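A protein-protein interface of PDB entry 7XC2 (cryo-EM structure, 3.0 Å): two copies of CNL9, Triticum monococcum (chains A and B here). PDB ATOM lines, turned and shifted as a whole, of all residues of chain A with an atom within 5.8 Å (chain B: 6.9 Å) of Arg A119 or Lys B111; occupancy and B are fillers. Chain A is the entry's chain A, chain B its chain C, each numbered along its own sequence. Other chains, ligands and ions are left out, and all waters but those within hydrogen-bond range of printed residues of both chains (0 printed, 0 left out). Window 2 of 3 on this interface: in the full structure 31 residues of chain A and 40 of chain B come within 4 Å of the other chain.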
ATOM      1  N   ALA A 114      13.458 -27.833 -28.388  1.00  0.00           N
ATOM      2  CA  ALA A 114      12.958 -27.717 -27.021  1.00  0.00           C
ATOM      3  C   ALA A 114      11.441 -27.588 -26.998  1.00  0.00           C
ATOM      4  O   ALA A 114      10.752 -28.284 -26.237  1.00  0.00           O
ATOM      5  CB  ALA A 114      13.601 -26.524 -26.328  1.00  0.00           C
ATOM      6  N   GLU A 115      10.901 -26.685 -27.818  1.00  0.00           N
ATOM      7  CA  GLU A 115       9.448 -26.543 -27.878  1.00  0.00           C
ATOM      8  C   GLU A 115       8.788 -27.849 -28.281  1.00  0.00           C
ATOM      9  O   GLU A 115       7.754 -28.238 -27.722  1.00  0.00           O
ATOM     10  CB  GLU A 115       9.060 -25.449 -28.861  1.00  0.00           C
ATOM     11  CG  GLU A 115       9.530 -24.079 -28.477  1.00  0.00           C
ATOM     12  CD  GLU A 115       9.195 -23.056 -29.534  1.00  0.00           C
ATOM     13  OE1 GLU A 115       8.648 -23.453 -30.582  1.00  0.00           O
ATOM     14  OE2 GLU A 115       9.478 -21.859 -29.322  1.00  0.00           O
ATOM     15  N   LEU A 116       9.371 -28.533 -29.260  1.00  0.00           N
ATOM     16  CA  LEU A 116       8.803 -29.788 -29.729  1.00  0.00           C
ATOM     17  C   LEU A 116       8.693 -30.796 -28.600  1.00  0.00           C
ATOM     18  O   LEU A 116       7.657 -31.443 -28.432  1.00  0.00           O
ATOM     19  CB  LEU A 116       9.655 -30.342 -30.859  1.00  0.00           C
ATOM     20  CG  LEU A 116       9.021 -31.484 -31.620  1.00  0.00           C
ATOM     21  CD1 LEU A 116       7.679 -31.037 -32.102  1.00  0.00           C
ATOM     22  CD2 LEU A 116       9.907 -31.842 -32.776  1.00  0.00           C
ATOM     23  N   ARG A 117       9.756 -30.949 -27.811  1.00  0.00           N
ATOM     24  CA  ARG A 117       9.677 -31.888 -26.699  1.00  0.00           C
ATOM     25  C   ARG A 117       8.609 -31.472 -25.707  1.00  0.00           C
ATOM     26  O   ARG A 117       7.834 -32.308 -25.235  1.00  0.00           O
ATOM     27  CB  ARG A 117      11.011 -32.014 -25.976  1.00  0.00           C
ATOM     28  CG  ARG A 117      10.879 -32.895 -24.753  1.00  0.00           C
ATOM     29  CD  ARG A 117      12.092 -32.867 -23.863  1.00  0.00           C
ATOM     30  NE  ARG A 117      12.273 -31.581 -23.211  1.00  0.00           N
ATOM     31  CZ  ARG A 117      12.787 -31.435 -21.998  1.00  0.00           C
ATOM     32  NH1 ARG A 117      13.157 -32.498 -21.304  1.00  0.00           N
ATOM     33  NH2 ARG A 117      12.923 -30.229 -21.476  1.00  0.00           N
ATOM     34  N   GLN A 118       8.555 -30.185 -25.368  1.00  0.00           N
ATOM     35  CA  GLN A 118       7.561 -29.749 -24.395  1.00  0.00           C
ATOM     36  C   GLN A 118       6.141 -29.992 -24.872  1.00  0.00           C
ATOM     37  O   GLN A 118       5.234 -30.125 -24.047  1.00  0.00           O
ATOM     38  CB  GLN A 118       7.738 -28.269 -24.076  1.00  0.00           C
ATOM     39  CG  GLN A 118       8.792 -28.005 -23.038  1.00  0.00           C
ATOM     40  CD  GLN A 118       8.511 -28.733 -21.751  1.00  0.00           C
ATOM     41  OE1 GLN A 118       7.370 -28.804 -21.304  1.00  0.00           O
ATOM     42  NE2 GLN A 118       9.551 -29.291 -21.147  1.00  0.00           N
ATOM     43  N   ARG A 119       5.928 -30.056 -26.182  1.00  0.00           N
ATOM     44  CA  ARG A 119       4.565 -30.096 -26.698  1.00  0.00           C
ATOM     45  C   ARG A 119       3.850 -31.401 -26.367  1.00  0.00           C
ATOM     46  O   ARG A 119       2.658 -31.387 -26.053  1.00  0.00           O
ATOM     47  CB  ARG A 119       4.588 -29.871 -28.201  1.00  0.00           C
ATOM     48  CG  ARG A 119       3.318 -29.334 -28.751  1.00  0.00           C
ATOM     49  CD  ARG A 119       3.503 -28.962 -30.188  1.00  0.00           C
ATOM     50  NE  ARG A 119       4.356 -27.797 -30.340  1.00  0.00           N
ATOM     51  CZ  ARG A 119       4.936 -27.453 -31.480  1.00  0.00           C
ATOM     52  NH1 ARG A 119       4.759 -28.195 -32.560  1.00  0.00           N
ATOM     53  NH2 ARG A 119       5.695 -26.373 -31.544  1.00  0.00           N
ATOM     54  N   TYR A 120       4.538 -32.540 -26.442  1.00  0.00           N
ATOM     55  CA  TYR A 120       3.884 -33.842 -26.352  1.00  0.00           C
ATOM     56  C   TYR A 120       4.335 -34.648 -25.145  1.00  0.00           C
ATOM     57  O   TYR A 120       4.400 -35.873 -25.207  1.00  0.00           O
ATOM     58  CB  TYR A 120       4.116 -34.656 -27.620  1.00  0.00           C
ATOM     59  CG  TYR A 120       3.600 -33.980 -28.843  1.00  0.00           C
ATOM     60  CD1 TYR A 120       2.248 -33.895 -29.083  1.00  0.00           C
ATOM     61  CD2 TYR A 120       4.462 -33.407 -29.749  1.00  0.00           C
ATOM     62  CE1 TYR A 120       1.770 -33.263 -30.190  1.00  0.00           C
ATOM     63  CE2 TYR A 120       3.993 -32.776 -30.860  1.00  0.00           C
ATOM     64  CZ  TYR A 120       2.646 -32.705 -31.077  1.00  0.00           C
ATOM     65  OH  TYR A 120       2.167 -32.073 -32.191  1.00  0.00           O
ATOM     66  N   GLU A 121       4.638 -33.994 -24.038  1.00  0.00           N
ATOM     67  CA  GLU A 121       5.073 -34.699 -22.845  1.00  0.00           C
ATOM     68  C   GLU A 121       3.875 -35.002 -21.959  1.00  0.00           C
ATOM     69  O   GLU A 121       3.111 -34.100 -21.610  1.00  0.00           O
ATOM     70  CB  GLU A 121       6.098 -33.870 -22.082  1.00  0.00           C
ATOM     71  CG  GLU A 121       6.864 -34.653 -21.057  1.00  0.00           C
ATOM     72  CD  GLU A 121       8.042 -33.878 -20.519  1.00  0.00           C
ATOM     73  OE1 GLU A 121       7.985 -32.631 -20.532  1.00  0.00           O
ATOM     74  OE2 GLU A 121       9.027 -34.513 -20.091  1.00  0.00           O
ATOM     75  N   GLU B  18       8.356 -34.585 -35.561  1.00  0.00           N
ATOM     76  CA  GLU B  18       7.161 -34.389 -34.751  1.00  0.00           C
ATOM     77  C   GLU B  18       6.221 -35.580 -34.853  1.00  0.00           C
ATOM     78  O   GLU B  18       5.589 -35.971 -33.866  1.00  0.00           O
ATOM     79  CB  GLU B  18       6.454 -33.110 -35.176  1.00  0.00           C
ATOM     80  CG  GLU B  18       5.275 -32.761 -34.316  1.00  0.00           C
ATOM     81  CD  GLU B  18       5.047 -31.274 -34.232  1.00  0.00           C
ATOM     82  OE1 GLU B  18       4.361 -30.827 -33.291  1.00  0.00           O
ATOM     83  OE2 GLU B  18       5.557 -30.546 -35.105  1.00  0.00           O
ATOM     84  N   TRP B  44      -7.621 -34.714 -25.445  1.00  0.00           N
ATOM     85  CA  TRP B  44      -6.376 -34.245 -26.032  1.00  0.00           C
ATOM     86  C   TRP B  44      -5.804 -35.278 -26.994  1.00  0.00           C
ATOM     87  O   TRP B  44      -5.278 -34.924 -28.056  1.00  0.00           O
ATOM     88  CB  TRP B  44      -5.396 -33.909 -24.914  1.00  0.00           C
ATOM     89  CG  TRP B  44      -4.045 -33.558 -25.369  1.00  0.00           C
ATOM     90  CD1 TRP B  44      -3.665 -32.420 -25.995  1.00  0.00           C
ATOM     91  CD2 TRP B  44      -2.873 -34.345 -25.215  1.00  0.00           C
ATOM     92  NE1 TRP B  44      -2.324 -32.451 -26.254  1.00  0.00           N
ATOM     93  CE2 TRP B  44      -1.815 -33.629 -25.783  1.00  0.00           C
ATOM     94  CE3 TRP B  44      -2.617 -35.594 -24.658  1.00  0.00           C
ATOM     95  CZ2 TRP B  44      -0.524 -34.116 -25.808  1.00  0.00           C
ATOM     96  CZ3 TRP B  44      -1.341 -36.074 -24.684  1.00  0.00           C
ATOM     97  CH2 TRP B  44      -0.307 -35.341 -25.253  1.00  0.00           C
ATOM     98  N   VAL B  48      -4.883 -34.881 -30.993  1.00  0.00           N
ATOM     99  CA  VAL B  48      -3.548 -35.195 -31.487  1.00  0.00           C
ATOM    100  C   VAL B  48      -3.629 -36.153 -32.664  1.00  0.00           C
ATOM    101  O   VAL B  48      -2.902 -36.010 -33.655  1.00  0.00           O
ATOM    102  CB  VAL B  48      -2.681 -35.762 -30.353  1.00  0.00           C
ATOM    103  CG1 VAL B  48      -1.439 -36.389 -30.909  1.00  0.00           C
ATOM    104  CG2 VAL B  48      -2.312 -34.670 -29.396  1.00  0.00           C
ATOM    105  N   LEU B  51      -4.503 -34.217 -35.850  1.00  0.00           N
ATOM    106  CA  LEU B  51      -3.350 -33.488 -36.369  1.00  0.00           C
ATOM    107  C   LEU B  51      -2.367 -34.422 -37.054  1.00  0.00           C
ATOM    108  O   LEU B  51      -1.765 -34.067 -38.078  1.00  0.00           O
ATOM    109  CB  LEU B  51      -2.644 -32.728 -35.259  1.00  0.00           C
ATOM    110  CG  LEU B  51      -3.286 -31.425 -34.840  1.00  0.00           C
ATOM    111  CD1 LEU B  51      -2.452 -30.797 -33.756  1.00  0.00           C
ATOM    112  CD2 LEU B  51      -3.371 -30.528 -36.039  1.00  0.00           C
ATOM    113  N   VAL B 106      -0.646 -25.872 -40.449  1.00  0.00           N
ATOM    114  CA  VAL B 106      -0.641 -26.988 -39.512  1.00  0.00           C
ATOM    115  C   VAL B 106       0.284 -26.705 -38.337  1.00  0.00           C
ATOM    116  O   VAL B 106      -0.005 -27.107 -37.199  1.00  0.00           O
ATOM    117  CB  VAL B 106      -0.285 -28.301 -40.228  1.00  0.00           C
ATOM    118  CG1 VAL B 106       1.176 -28.360 -40.553  1.00  0.00           C
ATOM    119  CG2 VAL B 106      -0.677 -29.472 -39.373  1.00  0.00           C
ATOM    120  N   VAL B 107       1.382 -25.981 -38.563  1.00  0.00           N
ATOM    121  CA  VAL B 107       2.242 -25.627 -37.437  1.00  0.00           C
ATOM    122  C   VAL B 107       1.486 -24.748 -36.452  1.00  0.00           C
ATOM    123  O   VAL B 107       1.561 -24.938 -35.225  1.00  0.00           O
ATOM    124  CB  VAL B 107       3.518 -24.941 -37.943  1.00  0.00           C
ATOM    125  CG1 VAL B 107       4.265 -24.328 -36.791  1.00  0.00           C
ATOM    126  CG2 VAL B 107       4.387 -25.939 -38.660  1.00  0.00           C
ATOM    127  N   LEU B 108       0.740 -23.775 -36.973  1.00  0.00           N
ATOM    128  CA  LEU B 108      -0.047 -22.912 -36.103  1.00  0.00           C
ATOM    129  C   LEU B 108      -1.041 -23.716 -35.276  1.00  0.00           C
ATOM    130  O   LEU B 108      -1.185 -23.489 -34.066  1.00  0.00           O
ATOM    131  CB  LEU B 108      -0.773 -21.868 -36.937  1.00  0.00           C
ATOM    132  CG  LEU B 108      -1.311 -20.688 -36.151  1.00  0.00           C
ATOM    133  CD1 LEU B 108      -0.164 -19.966 -35.490  1.00  0.00           C
ATOM    134  CD2 LEU B 108      -2.065 -19.765 -37.076  1.00  0.00           C
ATOM    135  N   GLN B 109      -1.737 -24.658 -35.910  1.00  0.00           N
ATOM    136  CA  GLN B 109      -2.722 -25.441 -35.171  1.00  0.00           C
ATOM    137  C   GLN B 109      -2.070 -26.259 -34.066  1.00  0.00           C
ATOM    138  O   GLN B 109      -2.632 -26.398 -32.970  1.00  0.00           O
ATOM    139  CB  GLN B 109      -3.491 -26.351 -36.114  1.00  0.00           C
ATOM    140  CG  GLN B 109      -4.360 -25.611 -37.087  1.00  0.00           C
ATOM    141  CD  GLN B 109      -5.087 -26.545 -38.015  1.00  0.00           C
ATOM    142  OE1 GLN B 109      -5.613 -26.133 -39.046  1.00  0.00           O
ATOM    143  NE2 GLN B 109      -5.123 -27.818 -37.656  1.00  0.00           N
ATOM    144  N   ALA B 110      -0.892 -26.819 -34.333  1.00  0.00           N
ATOM    145  CA  ALA B 110      -0.208 -27.592 -33.302  1.00  0.00           C
ATOM    146  C   ALA B 110       0.124 -26.727 -32.093  1.00  0.00           C
ATOM    147  O   ALA B 110      -0.121 -27.120 -30.941  1.00  0.00           O
ATOM    148  CB  ALA B 110       1.057 -28.221 -33.874  1.00  0.00           C
ATOM    149  N   LYS B 111       0.692 -25.543 -32.335  1.00  0.00           N
ATOM    150  CA  LYS B 111       0.988 -24.643 -31.222  1.00  0.00           C
ATOM    151  C   LYS B 111      -0.264 -24.325 -30.422  1.00  0.00           C
ATOM    152  O   LYS B 111      -0.243 -24.310 -29.181  1.00  0.00           O
ATOM    153  CB  LYS B 111       1.606 -23.350 -31.731  1.00  0.00           C
ATOM    154  CG  LYS B 111       3.026 -23.471 -32.181  1.00  0.00           C
ATOM    155  CD  LYS B 111       3.536 -22.137 -32.661  1.00  0.00           C
ATOM    156  CE  LYS B 111       4.898 -22.278 -33.306  1.00  0.00           C
ATOM    157  NZ  LYS B 111       5.291 -21.046 -34.037  1.00  0.00           N
ATOM    158  N   GLN B 112      -1.363 -24.056 -31.121  1.00  0.00           N
ATOM    159  CA  GLN B 112      -2.594 -23.682 -30.440  1.00  0.00           C
ATOM    160  C   GLN B 112      -3.091 -24.798 -29.537  1.00  0.00           C
ATOM    161  O   GLN B 112      -3.492 -24.551 -28.394  1.00  0.00           O
ATOM    162  CB  GLN B 112      -3.648 -23.316 -31.471  1.00  0.00           C
ATOM    163  CG  GLN B 112      -4.846 -22.628 -30.911  1.00  0.00           C
ATOM    164  CD  GLN B 112      -5.653 -21.965 -31.991  1.00  0.00           C
ATOM    165  OE1 GLN B 112      -5.102 -21.321 -32.883  1.00  0.00           O
ATOM    166  NE2 GLN B 112      -6.967 -22.126 -31.934  1.00  0.00           N
ATOM    167  N   LEU B 113      -3.071 -26.035 -30.029  1.00  0.00           N
ATOM    168  CA  LEU B 113      -3.530 -27.145 -29.203  1.00  0.00           C
ATOM    169  C   LEU B 113      -2.638 -27.330 -27.985  1.00  0.00           C
ATOM    170  O   LEU B 113      -3.120 -27.668 -26.896  1.00  0.00           O
ATOM    171  CB  LEU B 113      -3.582 -28.426 -30.024  1.00  0.00           C
ATOM    172  CG  LEU B 113      -3.859 -29.707 -29.247  1.00  0.00           C
ATOM    173  CD1 LEU B 113      -5.203 -29.632 -28.584  1.00  0.00           C
ATOM    174  CD2 LEU B 113      -3.801 -30.883 -30.174  1.00  0.00           C
ATOM    175  N   ALA B 114      -1.331 -27.115 -28.142  1.00  0.00           N
ATOM    176  CA  ALA B 114      -0.441 -27.234 -26.991  1.00  0.00           C
ATOM    177  C   ALA B 114      -0.804 -26.230 -25.906  1.00  0.00           C
ATOM    178  O   ALA B 114      -0.917 -26.582 -24.722  1.00  0.00           O
ATOM    179  CB  ALA B 114       1.005 -27.042 -27.428  1.00  0.00           C
ATOM    180  N   GLU B 115      -0.977 -24.964 -26.291  1.00  0.00           N
ATOM    181  CA  GLU B 115      -1.373 -23.960 -25.307  1.00  0.00           C
ATOM    182  C   GLU B 115      -2.689 -24.327 -24.649  1.00  0.00           C
ATOM    183  O   GLU B 115      -2.856 -24.178 -23.431  1.00  0.00           O
ATOM    184  CB  GLU B 115      -1.492 -22.592 -25.961  1.00  0.00           C
ATOM    185  CG  GLU B 115      -0.207 -22.055 -26.511  1.00  0.00           C
ATOM    186  CD  GLU B 115      -0.408 -20.742 -27.226  1.00  0.00           C
ATOM    187  OE1 GLU B 115      -1.571 -20.302 -27.328  1.00  0.00           O
ATOM    188  OE2 GLU B 115       0.588 -20.150 -27.688  1.00  0.00           O
ATOM    189  N   LEU B 116      -3.642 -24.803 -25.446  1.00  0.00           N
ATOM    190  CA  LEU B 116      -4.944 -25.168 -24.911  1.00  0.00           C
ATOM    191  C   LEU B 116      -4.818 -26.227 -23.832  1.00  0.00           C
ATOM    192  O   LEU B 116      -5.425 -26.113 -22.764  1.00  0.00           O
ATOM    193  CB  LEU B 116      -5.838 -25.658 -26.038  1.00  0.00           C
ATOM    194  CG  LEU B 116      -7.296 -25.795 -25.667  1.00  0.00           C
ATOM    195  CD1 LEU B 116      -7.764 -24.488 -25.114  1.00  0.00           C
ATOM    196  CD2 LEU B 116      -8.074 -26.159 -26.896  1.00  0.00           C
ATOM    197  N   ARG B 117      -4.031 -27.270 -24.088  1.00  0.00           N
ATOM    198  CA  ARG B 117      -3.862 -28.294 -23.064  1.00  0.00           C
ATOM    199  C   ARG B 117      -3.219 -27.717 -21.817  1.00  0.00           C
ATOM    200  O   ARG B 117      -3.652 -28.008 -20.698  1.00  0.00           O
ATOM    201  CB  ARG B 117      -3.024 -29.459 -23.566  1.00  0.00           C
ATOM    202  CG  ARG B 117      -2.755 -30.450 -22.455  1.00  0.00           C
ATOM    203  CD  ARG B 117      -1.736 -31.494 -22.819  1.00  0.00           C
ATOM    204  NE  ARG B 117      -0.402 -30.940 -22.969  1.00  0.00           N
ATOM    205  CZ  ARG B 117       0.708 -31.598 -22.664  1.00  0.00           C
ATOM    206  NH1 ARG B 117       0.637 -32.827 -22.181  1.00  0.00           N
ATOM    207  NH2 ARG B 117       1.886 -31.026 -22.836  1.00  0.00           N
ATOM    208  N   GLN B 118      -2.178 -26.905 -21.984  1.00  0.00           N
ATOM    209  CA  GLN B 118      -1.514 -26.352 -20.809  1.00  0.00           C
ATOM    210  C   GLN B 118      -2.440 -25.484 -19.976  1.00  0.00           C
ATOM    211  O   GLN B 118      -2.215 -25.332 -18.774  1.00  0.00           O
ATOM    212  CB  GLN B 118      -0.293 -25.537 -21.218  1.00  0.00           C
ATOM    213  CG  GLN B 118       0.932 -26.374 -21.453  1.00  0.00           C
ATOM    214  CD  GLN B 118       1.297 -27.191 -20.241  1.00  0.00           C
ATOM    215  OE1 GLN B 118       1.221 -26.711 -19.115  1.00  0.00           O
ATOM    216  NE2 GLN B 118       1.688 -28.437 -20.464  1.00  0.00           N
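NH1 of Arg A119 lies within salt-bridge range of OE1 of Glu B18 (2.8 Å). The side-chain carboxylate (OE1) of Glu B18 lies within hydrogen-bond range of the side-chain hydroxyl (OH) of Tyr A120 (2.8 Å). The backbone carbonyl oxygen (O) of Arg A119 sits at hydrogen-bond distance from the guanidinium group (NH2) of Arg B117 (3.3 Å). NH1 of Arg B117 is in hydrogen-bond range of O of Glu A121 (2.8 Å).
Leu A116 touches Glu B18. Gln A118 touches Arg B117. Arg A119 touches Ala B110. Arg A119 touches Lys B111 (NH2 to CG, 3.99 Å). Arg A119 touches Ala B114 (CG to CB, 3.5 Å).
Of the printed residues of chain B, Arg A119 touches Glu B18, Ala B110, Lys B111, Ala B114 and Arg B117. Printed residues of chain B within 4 Å of Glu A121: Arg B117. Printed residues of chain A within 4 Å of Glu B18: Leu A116 (3.4 Å), Arg A119 (2.8 Å) and Tyr A120 (2.8 Å). Leu B108 touches none of the printed residues of chain A. Of the printed residues of chain A, Ala B110 touches Arg A119. Printed residues of chain A within 4 Å of Lys B111: Arg A119 (3.99 Å). Leu B113 touches none of the printed residues of chain A.
Of the 17 printed residues of chain B, 5 touch a printed residue of chain A. Hydrophobic or aromatic side chains of chain B within 4 Å of the printed part of chain A: Ala B110 and Ala B114. Along chain A the printed residues that touch a printed residue of chain B span positions 116 to 121. Among the printed residues, 9 pairs touch across the chains. Among the printed residues, Asp or Glu carboxylates within 4 Å of a Lys or Arg side-chain nitrogen of the other chain: Arg A119 with Glu B18.
Gln A118 touches Arg B117, but with the chains exchanged Arg A117 does not touch Gln B118 (8.7 Å).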
